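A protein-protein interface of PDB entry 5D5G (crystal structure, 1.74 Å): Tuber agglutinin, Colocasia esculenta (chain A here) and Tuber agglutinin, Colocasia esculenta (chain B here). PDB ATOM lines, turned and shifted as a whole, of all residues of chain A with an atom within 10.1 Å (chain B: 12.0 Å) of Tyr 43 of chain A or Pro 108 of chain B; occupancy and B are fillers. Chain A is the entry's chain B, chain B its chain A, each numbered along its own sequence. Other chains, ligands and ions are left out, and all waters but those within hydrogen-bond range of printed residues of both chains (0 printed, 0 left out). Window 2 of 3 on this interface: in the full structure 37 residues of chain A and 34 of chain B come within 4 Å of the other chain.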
ATOM      1  N   SER A  25     -18.367 -31.812  -7.276  1.00  0.00           N
ATOM      2  CA  SER A  25     -19.140 -32.067  -6.076  1.00  0.00           C
ATOM      3  C   SER A  25     -20.392 -31.174  -6.009  1.00  0.00           C
ATOM      4  O   SER A  25     -20.904 -30.879  -4.920  1.00  0.00           O
ATOM      5  CB  SER A  25     -18.238 -31.810  -4.867  1.00  0.00           C
ATOM      6  OG  SER A  25     -18.782 -32.358  -3.685  1.00  0.00           O
ATOM      7  N   HIS A  26     -20.884 -30.737  -7.169  1.00  0.00           N
ATOM      8  CA  HIS A  26     -22.033 -29.823  -7.206  1.00  0.00           C
ATOM      9  C   HIS A  26     -23.076 -30.223  -8.238  1.00  0.00           C
ATOM     10  O   HIS A  26     -22.765 -30.811  -9.278  1.00  0.00           O
ATOM     11  CB  HIS A  26     -21.584 -28.395  -7.529  1.00  0.00           C
ATOM     12  CG  HIS A  26     -20.256 -28.024  -6.947  1.00  0.00           C
ATOM     13  ND1 HIS A  26     -19.998 -28.067  -5.593  1.00  0.00           N
ATOM     14  CD2 HIS A  26     -19.116 -27.588  -7.536  1.00  0.00           C
ATOM     15  CE1 HIS A  26     -18.752 -27.682  -5.373  1.00  0.00           C
ATOM     16  NE2 HIS A  26     -18.196 -27.385  -6.534  1.00  0.00           N
ATOM     17  N   GLN A  27     -24.328 -29.886  -7.962  1.00  0.00           N
ATOM     18  CA  GLN A  27     -25.328 -29.954  -9.003  1.00  0.00           C
ATOM     19  C   GLN A  27     -26.245 -28.749  -8.873  1.00  0.00           C
ATOM     20  O   GLN A  27     -26.380 -28.177  -7.792  1.00  0.00           O
ATOM     21  CB  GLN A  27     -26.129 -31.259  -8.928  1.00  0.00           C
ATOM     22  CG  GLN A  27     -25.474 -32.348  -8.098  1.00  0.00           C
ATOM     23  CD  GLN A  27     -26.444 -33.446  -7.728  1.00  0.00           C
ATOM     24  OE1 GLN A  27     -27.258 -33.866  -8.548  1.00  0.00           O
ATOM     25  NE2 GLN A  27     -26.370 -33.912  -6.484  1.00  0.00           N
ATOM     26  N   VAL A  37     -32.749 -25.953  -7.477  1.00  0.00           N
ATOM     27  CA  VAL A  37     -31.842 -26.182  -6.366  1.00  0.00           C
ATOM     28  C   VAL A  37     -30.405 -26.396  -6.804  1.00  0.00           C
ATOM     29  O   VAL A  37     -30.118 -27.186  -7.703  1.00  0.00           O
ATOM     30  CB  VAL A  37     -32.258 -27.409  -5.564  1.00  0.00           C
ATOM     31  CG1 VAL A  37     -31.735 -27.294  -4.140  1.00  0.00           C
ATOM     32  CG2 VAL A  37     -33.780 -27.562  -5.582  1.00  0.00           C
ATOM     33  N   LEU A  38     -29.507 -25.684  -6.143  1.00  0.00           N
ATOM     34  CA  LEU A  38     -28.088 -25.849  -6.357  1.00  0.00           C
ATOM     35  C   LEU A  38     -27.566 -26.593  -5.162  1.00  0.00           C
ATOM     36  O   LEU A  38     -27.493 -26.044  -4.066  1.00  0.00           O
ATOM     37  CB  LEU A  38     -27.405 -24.481  -6.419  1.00  0.00           C
ATOM     38  CG  LEU A  38     -25.882 -24.484  -6.568  1.00  0.00           C
ATOM     39  CD1 LEU A  38     -25.478 -24.944  -7.962  1.00  0.00           C
ATOM     40  CD2 LEU A  38     -25.294 -23.103  -6.272  1.00  0.00           C
ATOM     41  N   TYR A  39     -27.225 -27.855  -5.349  1.00  0.00           N
ATOM     42  CA  TYR A  39     -26.576 -28.559  -4.277  1.00  0.00           C
ATOM     43  C   TYR A  39     -25.122 -28.342  -4.569  1.00  0.00           C
ATOM     44  O   TYR A  39     -24.660 -28.673  -5.657  1.00  0.00           O
ATOM     45  CB  TYR A  39     -26.944 -30.034  -4.303  1.00  0.00           C
ATOM     46  CG  TYR A  39     -28.438 -30.264  -4.231  1.00  0.00           C
ATOM     47  CD1 TYR A  39     -29.093 -30.366  -3.007  1.00  0.00           C
ATOM     48  CD2 TYR A  39     -29.193 -30.365  -5.391  1.00  0.00           C
ATOM     49  CE1 TYR A  39     -30.462 -30.571  -2.948  1.00  0.00           C
ATOM     50  CE2 TYR A  39     -30.564 -30.570  -5.341  1.00  0.00           C
ATOM     51  CZ  TYR A  39     -31.198 -30.674  -4.120  1.00  0.00           C
ATOM     52  OH  TYR A  39     -32.577 -30.881  -4.086  1.00  0.00           O
ATOM     53  N   GLY A  40     -24.418 -27.742  -3.614  1.00  0.00           N
ATOM     54  CA  GLY A  40     -23.036 -27.346  -3.821  1.00  0.00           C
ATOM     55  C   GLY A  40     -22.640 -26.212  -2.894  1.00  0.00           C
ATOM     56  O   GLY A  40     -23.418 -25.823  -2.016  1.00  0.00           O
ATOM     57  N   GLY A  41     -21.435 -25.683  -3.089  1.00  0.00           N
ATOM     58  CA  GLY A  41     -20.904 -24.638  -2.230  1.00  0.00           C
ATOM     59  C   GLY A  41     -20.947 -25.078  -0.787  1.00  0.00           C
ATOM     60  O   GLY A  41     -21.066 -26.258  -0.503  1.00  0.00           O
ATOM     61  N   LYS A  42     -20.864 -24.147   0.146  1.00  0.00           N
ATOM     62  CA  LYS A  42     -21.010 -24.571   1.511  1.00  0.00           C
ATOM     63  C   LYS A  42     -22.481 -24.823   1.851  1.00  0.00           C
ATOM     64  O   LYS A  42     -22.808 -25.829   2.469  1.00  0.00           O
ATOM     65  CB  LYS A  42     -20.387 -23.568   2.461  1.00  0.00           C
ATOM     66  CG  LYS A  42     -20.493 -23.974   3.899  1.00  0.00           C
ATOM     67  CD  LYS A  42     -19.269 -23.543   4.631  1.00  0.00           C
ATOM     68  CE  LYS A  42     -19.270 -23.994   6.067  1.00  0.00           C
ATOM     69  NZ  LYS A  42     -17.880 -23.869   6.599  1.00  0.00           N
ATOM     70  N   TYR A  43     -23.366 -23.928   1.420  1.00  0.00           N
ATOM     71  CA  TYR A  43     -24.746 -23.916   1.888  1.00  0.00           C
ATOM     72  C   TYR A  43     -25.780 -24.190   0.796  1.00  0.00           C
ATOM     73  O   TYR A  43     -26.972 -24.244   1.074  1.00  0.00           O
ATOM     74  CB  TYR A  43     -25.044 -22.559   2.511  1.00  0.00           C
ATOM     75  CG  TYR A  43     -24.180 -22.183   3.694  1.00  0.00           C
ATOM     76  CD1 TYR A  43     -24.285 -22.866   4.895  1.00  0.00           C
ATOM     77  CD2 TYR A  43     -23.288 -21.115   3.624  1.00  0.00           C
ATOM     78  CE1 TYR A  43     -23.510 -22.519   5.984  1.00  0.00           C
ATOM     79  CE2 TYR A  43     -22.525 -20.758   4.718  1.00  0.00           C
ATOM     80  CZ  TYR A  43     -22.639 -21.466   5.892  1.00  0.00           C
ATOM     81  OH  TYR A  43     -21.880 -21.116   6.998  1.00  0.00           O
ATOM     82  N   GLY A  44     -25.340 -24.346  -0.445  1.00  0.00           N
ATOM     83  CA  GLY A  44     -26.256 -24.581  -1.548  1.00  0.00           C
ATOM     84  C   GLY A  44     -27.159 -23.389  -1.810  1.00  0.00           C
ATOM     85  O   GLY A  44     -26.869 -22.285  -1.362  1.00  0.00           O
ATOM     86  N   TRP A  45     -28.253 -23.613  -2.537  1.00  0.00           N
ATOM     87  CA  TRP A  45     -29.202 -22.557  -2.901  1.00  0.00           C
ATOM     88  C   TRP A  45     -30.443 -23.096  -3.598  1.00  0.00           C
ATOM     89  O   TRP A  45     -30.404 -24.172  -4.200  1.00  0.00           O
ATOM     90  CB  TRP A  45     -28.544 -21.550  -3.831  1.00  0.00           C
ATOM     91  CG  TRP A  45     -29.506 -20.571  -4.396  1.00  0.00           C
ATOM     92  CD1 TRP A  45     -30.024 -19.470  -3.775  1.00  0.00           C
ATOM     93  CD2 TRP A  45     -30.074 -20.597  -5.703  1.00  0.00           C
ATOM     94  NE1 TRP A  45     -30.884 -18.802  -4.623  1.00  0.00           N
ATOM     95  CE2 TRP A  45     -30.928 -19.478  -5.814  1.00  0.00           C
ATOM     96  CE3 TRP A  45     -29.951 -21.461  -6.789  1.00  0.00           C
ATOM     97  CZ2 TRP A  45     -31.634 -19.200  -6.973  1.00  0.00           C
ATOM     98  CZ3 TRP A  45     -30.655 -21.190  -7.932  1.00  0.00           C
ATOM     99  CH2 TRP A  45     -31.484 -20.067  -8.022  1.00  0.00           C
ATOM    100  N   GLN A  46     -31.542 -22.339  -3.528  1.00  0.00           N
ATOM    101  CA  GLN A  46     -32.763 -22.698  -4.241  1.00  0.00           C
ATOM    102  C   GLN A  46     -33.622 -21.505  -4.632  1.00  0.00           C
ATOM    103  O   GLN A  46     -33.708 -20.516  -3.905  1.00  0.00           O
ATOM    104  CB  GLN A  46     -33.604 -23.621  -3.390  1.00  0.00           C
ATOM    105  CG  GLN A  46     -33.979 -23.016  -2.079  1.00  0.00           C
ATOM    106  CD  GLN A  46     -35.257 -23.606  -1.563  1.00  0.00           C
ATOM    107  OE1 GLN A  46     -35.513 -24.802  -1.709  1.00  0.00           O
ATOM    108  NE2 GLN A  46     -36.083 -22.772  -0.981  1.00  0.00           N
ATOM    109  N   ASP A  95     -15.865 -23.941  -8.434  1.00  0.00           N
ATOM    110  CA  ASP A  95     -16.020 -23.326  -7.104  1.00  0.00           C
ATOM    111  C   ASP A  95     -17.445 -23.404  -6.572  1.00  0.00           C
ATOM    112  O   ASP A  95     -17.711 -23.040  -5.426  1.00  0.00           O
ATOM    113  CB  ASP A  95     -15.513 -21.874  -7.051  1.00  0.00           C
ATOM    114  CG  ASP A  95     -15.837 -21.095  -8.298  1.00  0.00           C
ATOM    115  OD1 ASP A  95     -16.873 -21.396  -8.926  1.00  0.00           O
ATOM    116  OD2 ASP A  95     -15.047 -20.190  -8.648  1.00  0.00           O
ATOM    117  N   GLY A  96     -18.358 -23.897  -7.399  1.00  0.00           N
ATOM    118  CA  GLY A  96     -19.720 -24.107  -6.952  1.00  0.00           C
ATOM    119  C   GLY A  96     -20.613 -22.923  -7.267  1.00  0.00           C
ATOM    120  O   GLY A  96     -21.823 -22.961  -7.061  1.00  0.00           O
ATOM    121  N   PHE A  97     -20.017 -21.856  -7.768  1.00  0.00           N
ATOM    122  CA  PHE A  97     -20.798 -20.729  -8.213  1.00  0.00           C
ATOM    123  C   PHE A  97     -21.477 -21.142  -9.488  1.00  0.00           C
ATOM    124  O   PHE A  97     -20.936 -21.931 -10.260  1.00  0.00           O
ATOM    125  CB  PHE A  97     -19.900 -19.531  -8.488  1.00  0.00           C
ATOM    126  CG  PHE A  97     -19.477 -18.810  -7.257  1.00  0.00           C
ATOM    127  CD1 PHE A  97     -18.977 -19.497  -6.175  1.00  0.00           C
ATOM    128  CD2 PHE A  97     -19.586 -17.445  -7.178  1.00  0.00           C
ATOM    129  CE1 PHE A  97     -18.591 -18.840  -5.042  1.00  0.00           C
ATOM    130  CE2 PHE A  97     -19.199 -16.784  -6.037  1.00  0.00           C
ATOM    131  CZ  PHE A  97     -18.700 -17.492  -4.968  1.00  0.00           C
ATOM    132  N   LYS B 102     -25.123 -13.889 -10.933  1.00  0.00           N
ATOM    133  CA  LYS B 102     -24.276 -14.769 -10.122  1.00  0.00           C
ATOM    134  C   LYS B 102     -25.000 -15.402  -8.916  1.00  0.00           C
ATOM    135  O   LYS B 102     -25.641 -14.698  -8.141  1.00  0.00           O
ATOM    136  CB  LYS B 102     -23.059 -13.986  -9.637  1.00  0.00           C
ATOM    137  CG  LYS B 102     -22.576 -14.331  -8.234  1.00  0.00           C
ATOM    138  CD  LYS B 102     -21.801 -13.151  -7.641  1.00  0.00           C
ATOM    139  CE  LYS B 102     -21.716 -13.210  -6.111  1.00  0.00           C
ATOM    140  NZ  LYS B 102     -21.344 -11.885  -5.503  1.00  0.00           N
ATOM    141  N   ILE B 103     -24.894 -16.727  -8.771  1.00  0.00           N
ATOM    142  CA  ILE B 103     -25.428 -17.475  -7.621  1.00  0.00           C
ATOM    143  C   ILE B 103     -24.317 -17.976  -6.709  1.00  0.00           C
ATOM    144  O   ILE B 103     -23.435 -18.708  -7.160  1.00  0.00           O
ATOM    145  CB  ILE B 103     -26.191 -18.732  -8.078  1.00  0.00           C
ATOM    146  CG1 ILE B 103     -27.255 -18.362  -9.110  1.00  0.00           C
ATOM    147  CG2 ILE B 103     -26.760 -19.487  -6.876  1.00  0.00           C
ATOM    148  CD1 ILE B 103     -28.259 -19.460  -9.417  1.00  0.00           C
ATOM    149  N   ASP B 104     -24.386 -17.635  -5.426  1.00  0.00           N
ATOM    150  CA  ASP B 104     -23.258 -17.821  -4.515  1.00  0.00           C
ATOM    151  C   ASP B 104     -23.653 -18.684  -3.321  1.00  0.00           C
ATOM    152  O   ASP B 104     -24.147 -18.172  -2.320  1.00  0.00           O
ATOM    153  CB  ASP B 104     -22.727 -16.437  -4.080  1.00  0.00           C
ATOM    154  CG  ASP B 104     -21.553 -16.503  -3.096  1.00  0.00           C
ATOM    155  OD1 ASP B 104     -21.647 -17.203  -2.070  1.00  0.00           O
ATOM    156  OD2 ASP B 104     -20.537 -15.808  -3.327  1.00  0.00           O
ATOM    157  N   PRO B 105     -23.420 -20.006  -3.418  1.00  0.00           N
ATOM    158  CA  PRO B 105     -23.705 -20.960  -2.339  1.00  0.00           C
ATOM    159  C   PRO B 105     -22.700 -20.839  -1.210  1.00  0.00           C
ATOM    160  O   PRO B 105     -22.740 -21.620  -0.255  1.00  0.00           O
ATOM    161  CB  PRO B 105     -23.529 -22.304  -3.022  1.00  0.00           C
ATOM    162  CG  PRO B 105     -22.538 -22.028  -4.094  1.00  0.00           C
ATOM    163  CD  PRO B 105     -22.922 -20.685  -4.621  1.00  0.00           C
ATOM    164  N   TRP B 106     -21.809 -19.862  -1.328  1.00  0.00           N
ATOM    165  CA  TRP B 106     -20.717 -19.667  -0.385  1.00  0.00           C
ATOM    166  C   TRP B 106     -20.894 -18.385   0.403  1.00  0.00           C
ATOM    167  O   TRP B 106     -19.938 -17.635   0.596  1.00  0.00           O
ATOM    168  CB  TRP B 106     -19.395 -19.548  -1.149  1.00  0.00           C
ATOM    169  CG  TRP B 106     -18.899 -20.810  -1.801  1.00  0.00           C
ATOM    170  CD1 TRP B 106     -19.059 -21.185  -3.105  1.00  0.00           C
ATOM    171  CD2 TRP B 106     -18.141 -21.842  -1.175  1.00  0.00           C
ATOM    172  NE1 TRP B 106     -18.445 -22.394  -3.331  1.00  0.00           N
ATOM    173  CE2 TRP B 106     -17.879 -22.822  -2.157  1.00  0.00           C
ATOM    174  CE3 TRP B 106     -17.668 -22.040   0.125  1.00  0.00           C
ATOM    175  CZ2 TRP B 106     -17.168 -23.973  -1.881  1.00  0.00           C
ATOM    176  CZ3 TRP B 106     -16.962 -23.179   0.398  1.00  0.00           C
ATOM    177  CH2 TRP B 106     -16.717 -24.139  -0.598  1.00  0.00           C
ATOM    178  N   VAL B 107     -22.110 -18.098   0.834  1.00  0.00           N
ATOM    179  CA  VAL B 107     -22.331 -16.907   1.638  1.00  0.00           C
ATOM    180  C   VAL B 107     -23.390 -17.233   2.663  1.00  0.00           C
ATOM    181  O   VAL B 107     -24.402 -17.836   2.330  1.00  0.00           O
ATOM    182  CB  VAL B 107     -22.743 -15.705   0.775  1.00  0.00           C
ATOM    183  CG1 VAL B 107     -23.922 -16.053  -0.109  1.00  0.00           C
ATOM    184  CG2 VAL B 107     -23.067 -14.511   1.645  1.00  0.00           C
ATOM    185  N   PRO B 108     -23.133 -16.884   3.927  1.00  0.00           N
ATOM    186  CA  PRO B 108     -24.062 -17.198   5.015  1.00  0.00           C
ATOM    187  C   PRO B 108     -25.283 -16.287   4.993  1.00  0.00           C
ATOM    188  O   PRO B 108     -26.375 -16.702   5.397  1.00  0.00           O
ATOM    189  CB  PRO B 108     -23.228 -16.943   6.271  1.00  0.00           C
ATOM    190  CG  PRO B 108     -22.193 -15.974   5.842  1.00  0.00           C
ATOM    191  CD  PRO B 108     -21.877 -16.302   4.422  1.00  0.00           C
ATOM    192  N   GLY B 109     -25.096 -15.061   4.517  1.00  0.00           N
ATOM    193  CA  GLY B 109     -26.192 -14.117   4.396  1.00  0.00           C
ATOM    194  C   GLY B 109     -26.008 -13.178   3.219  1.00  0.00           C
ATOM    195  O   GLY B 109     -26.875 -13.078   2.346  1.00  0.00           O
ATOM    196  OXT GLY B 109     -24.983 -12.498   3.109  1.00  0.00           O
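The backbone carbonyl oxygen of Asp 95 of chain A lies close to the indole nitrogen of Trp 106 of chain B (2.3 Å). The backbone carbonyl oxygen of Pro 105 of chain B is in hydrogen-bond range of the backbone NH of Tyr 43 of chain A. The backbone carbonyl oxygen (O) of Pro 105 of chain B is in hydrogen-bond range of the backbone NH (N) of Lys 42 of chain A.
Hydrophobic or aromatic side chains of chain B that line the printed part of chain A: Ile 103, Pro 105 and Trp 106. Hydrophobic or aromatic side chains of chain A that line the printed part of chain B: Leu 38, Tyr 43, Trp 45 and Phe 97. Among the printed residues, 17 pairs touch across the chains. Among the printed residues, no Asp or Glu carboxylate lies within 4 Å of a Lys or Arg side-chain nitrogen of the other chain.
Among the printed residues, pairs that only touch across the chains: Leu 38 of chain A with Ile 103 of chain B (3.9 Å), Leu 38 of chain A with Pro 105 of chain B (3.7 Å), Gly 40 of chain A with Pro 105 of chain B (3.7 Å), Gly 41 of chain A with Pro 105 of chain B (3.6 Å), Gly 41 of chain A with Trp 106 of chain B (3.5 Å), Lys 42 of chain A with Trp 106 of chain B (3.8 Å), Tyr 43 of chain A with Val 107 of chain B (3.7 Å), Tyr 43 of chain A with Pro 108 of chain B (3.9 Å), Gly 44 of chain A with Pro 105 of chain B (3.6 Å), Trp 45 of chain A with Ile 103 of chain B (3.3 Å), Gly 96 of chain A with Pro 105 of chain B (3.2 Å), Phe 97 of chain A with Ile 103 of chain B (3.5 Å), Phe 97 of chain A with Asp 104 of chain B (3.0 Å) and Phe 97 of chain A with Trp 106 of chain B (3.1 Å).
Tyr 43 of chain A touches just these residues of chain B: Pro 105, Val 107 and Pro 108. Pro 108 of chain B touches one residue of chain A. Gly 40 of chain A touches one residue of chain B. Of chain B, only Pro 105 and Trp 106 come within 4 Å of Gly 41 of chain A. Of chain B, only Pro 105 (3.2 Å) and Trp 106 (3.8 Å) come within 4 Å of Lys 42 of chain A. Gly 44 of chain A touches just one residue of chain B: Pro 105. Of chain A, only Tyr 43 comes within 4 Å of Val 107 of chain B. No residue of chain A comes within 4 Å of Gly 109 of chain B. Of the printed residues of chain A, Trp 106 of chain B touches Gly 41, Lys 42, Asp 95 and Phe 97. Of the printed residues of chain B, Trp 45 of chain A touches Ile 103. Of the printed residues of chain A, Ile 103 of chain B touches Leu 38 (3.9 Å), Trp 45 (3.3 Å) and Phe 97 (3.5 Å). Of the printed residues of chain B, Phe 97 of chain A touches Ile 103, Asp 104 and Trp 106. Printed residues of chain B within 4 Å of Asp 95 of chain A: Trp 106 (2.3 Å). The nearest printed residue of chain B that does not touch Leu 38 of chain A is Asp 104 of chain B (5.6 Å).
The backbone NH of Leu 38 of chain A lies within hydrogen-bond range of the backbone carbonyl oxygen of Trp 45 of chain A, at 2.6 Å. The side-chain carboxylate (OD1) of Asp 95 of chain A lies close to the backbone NH (N) of Phe 97 of chain A (3.4 Å). The side-chain carboxylate (OD1) of Asp 104 of chain B is in hydrogen-bond range of the backbone NH (N) of Trp 106 of chain B (2.8 Å). OD1 of Asp 104 of chain B sits at hydrogen-bond distance from N of Val 107 of chain B (3.1 Å).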
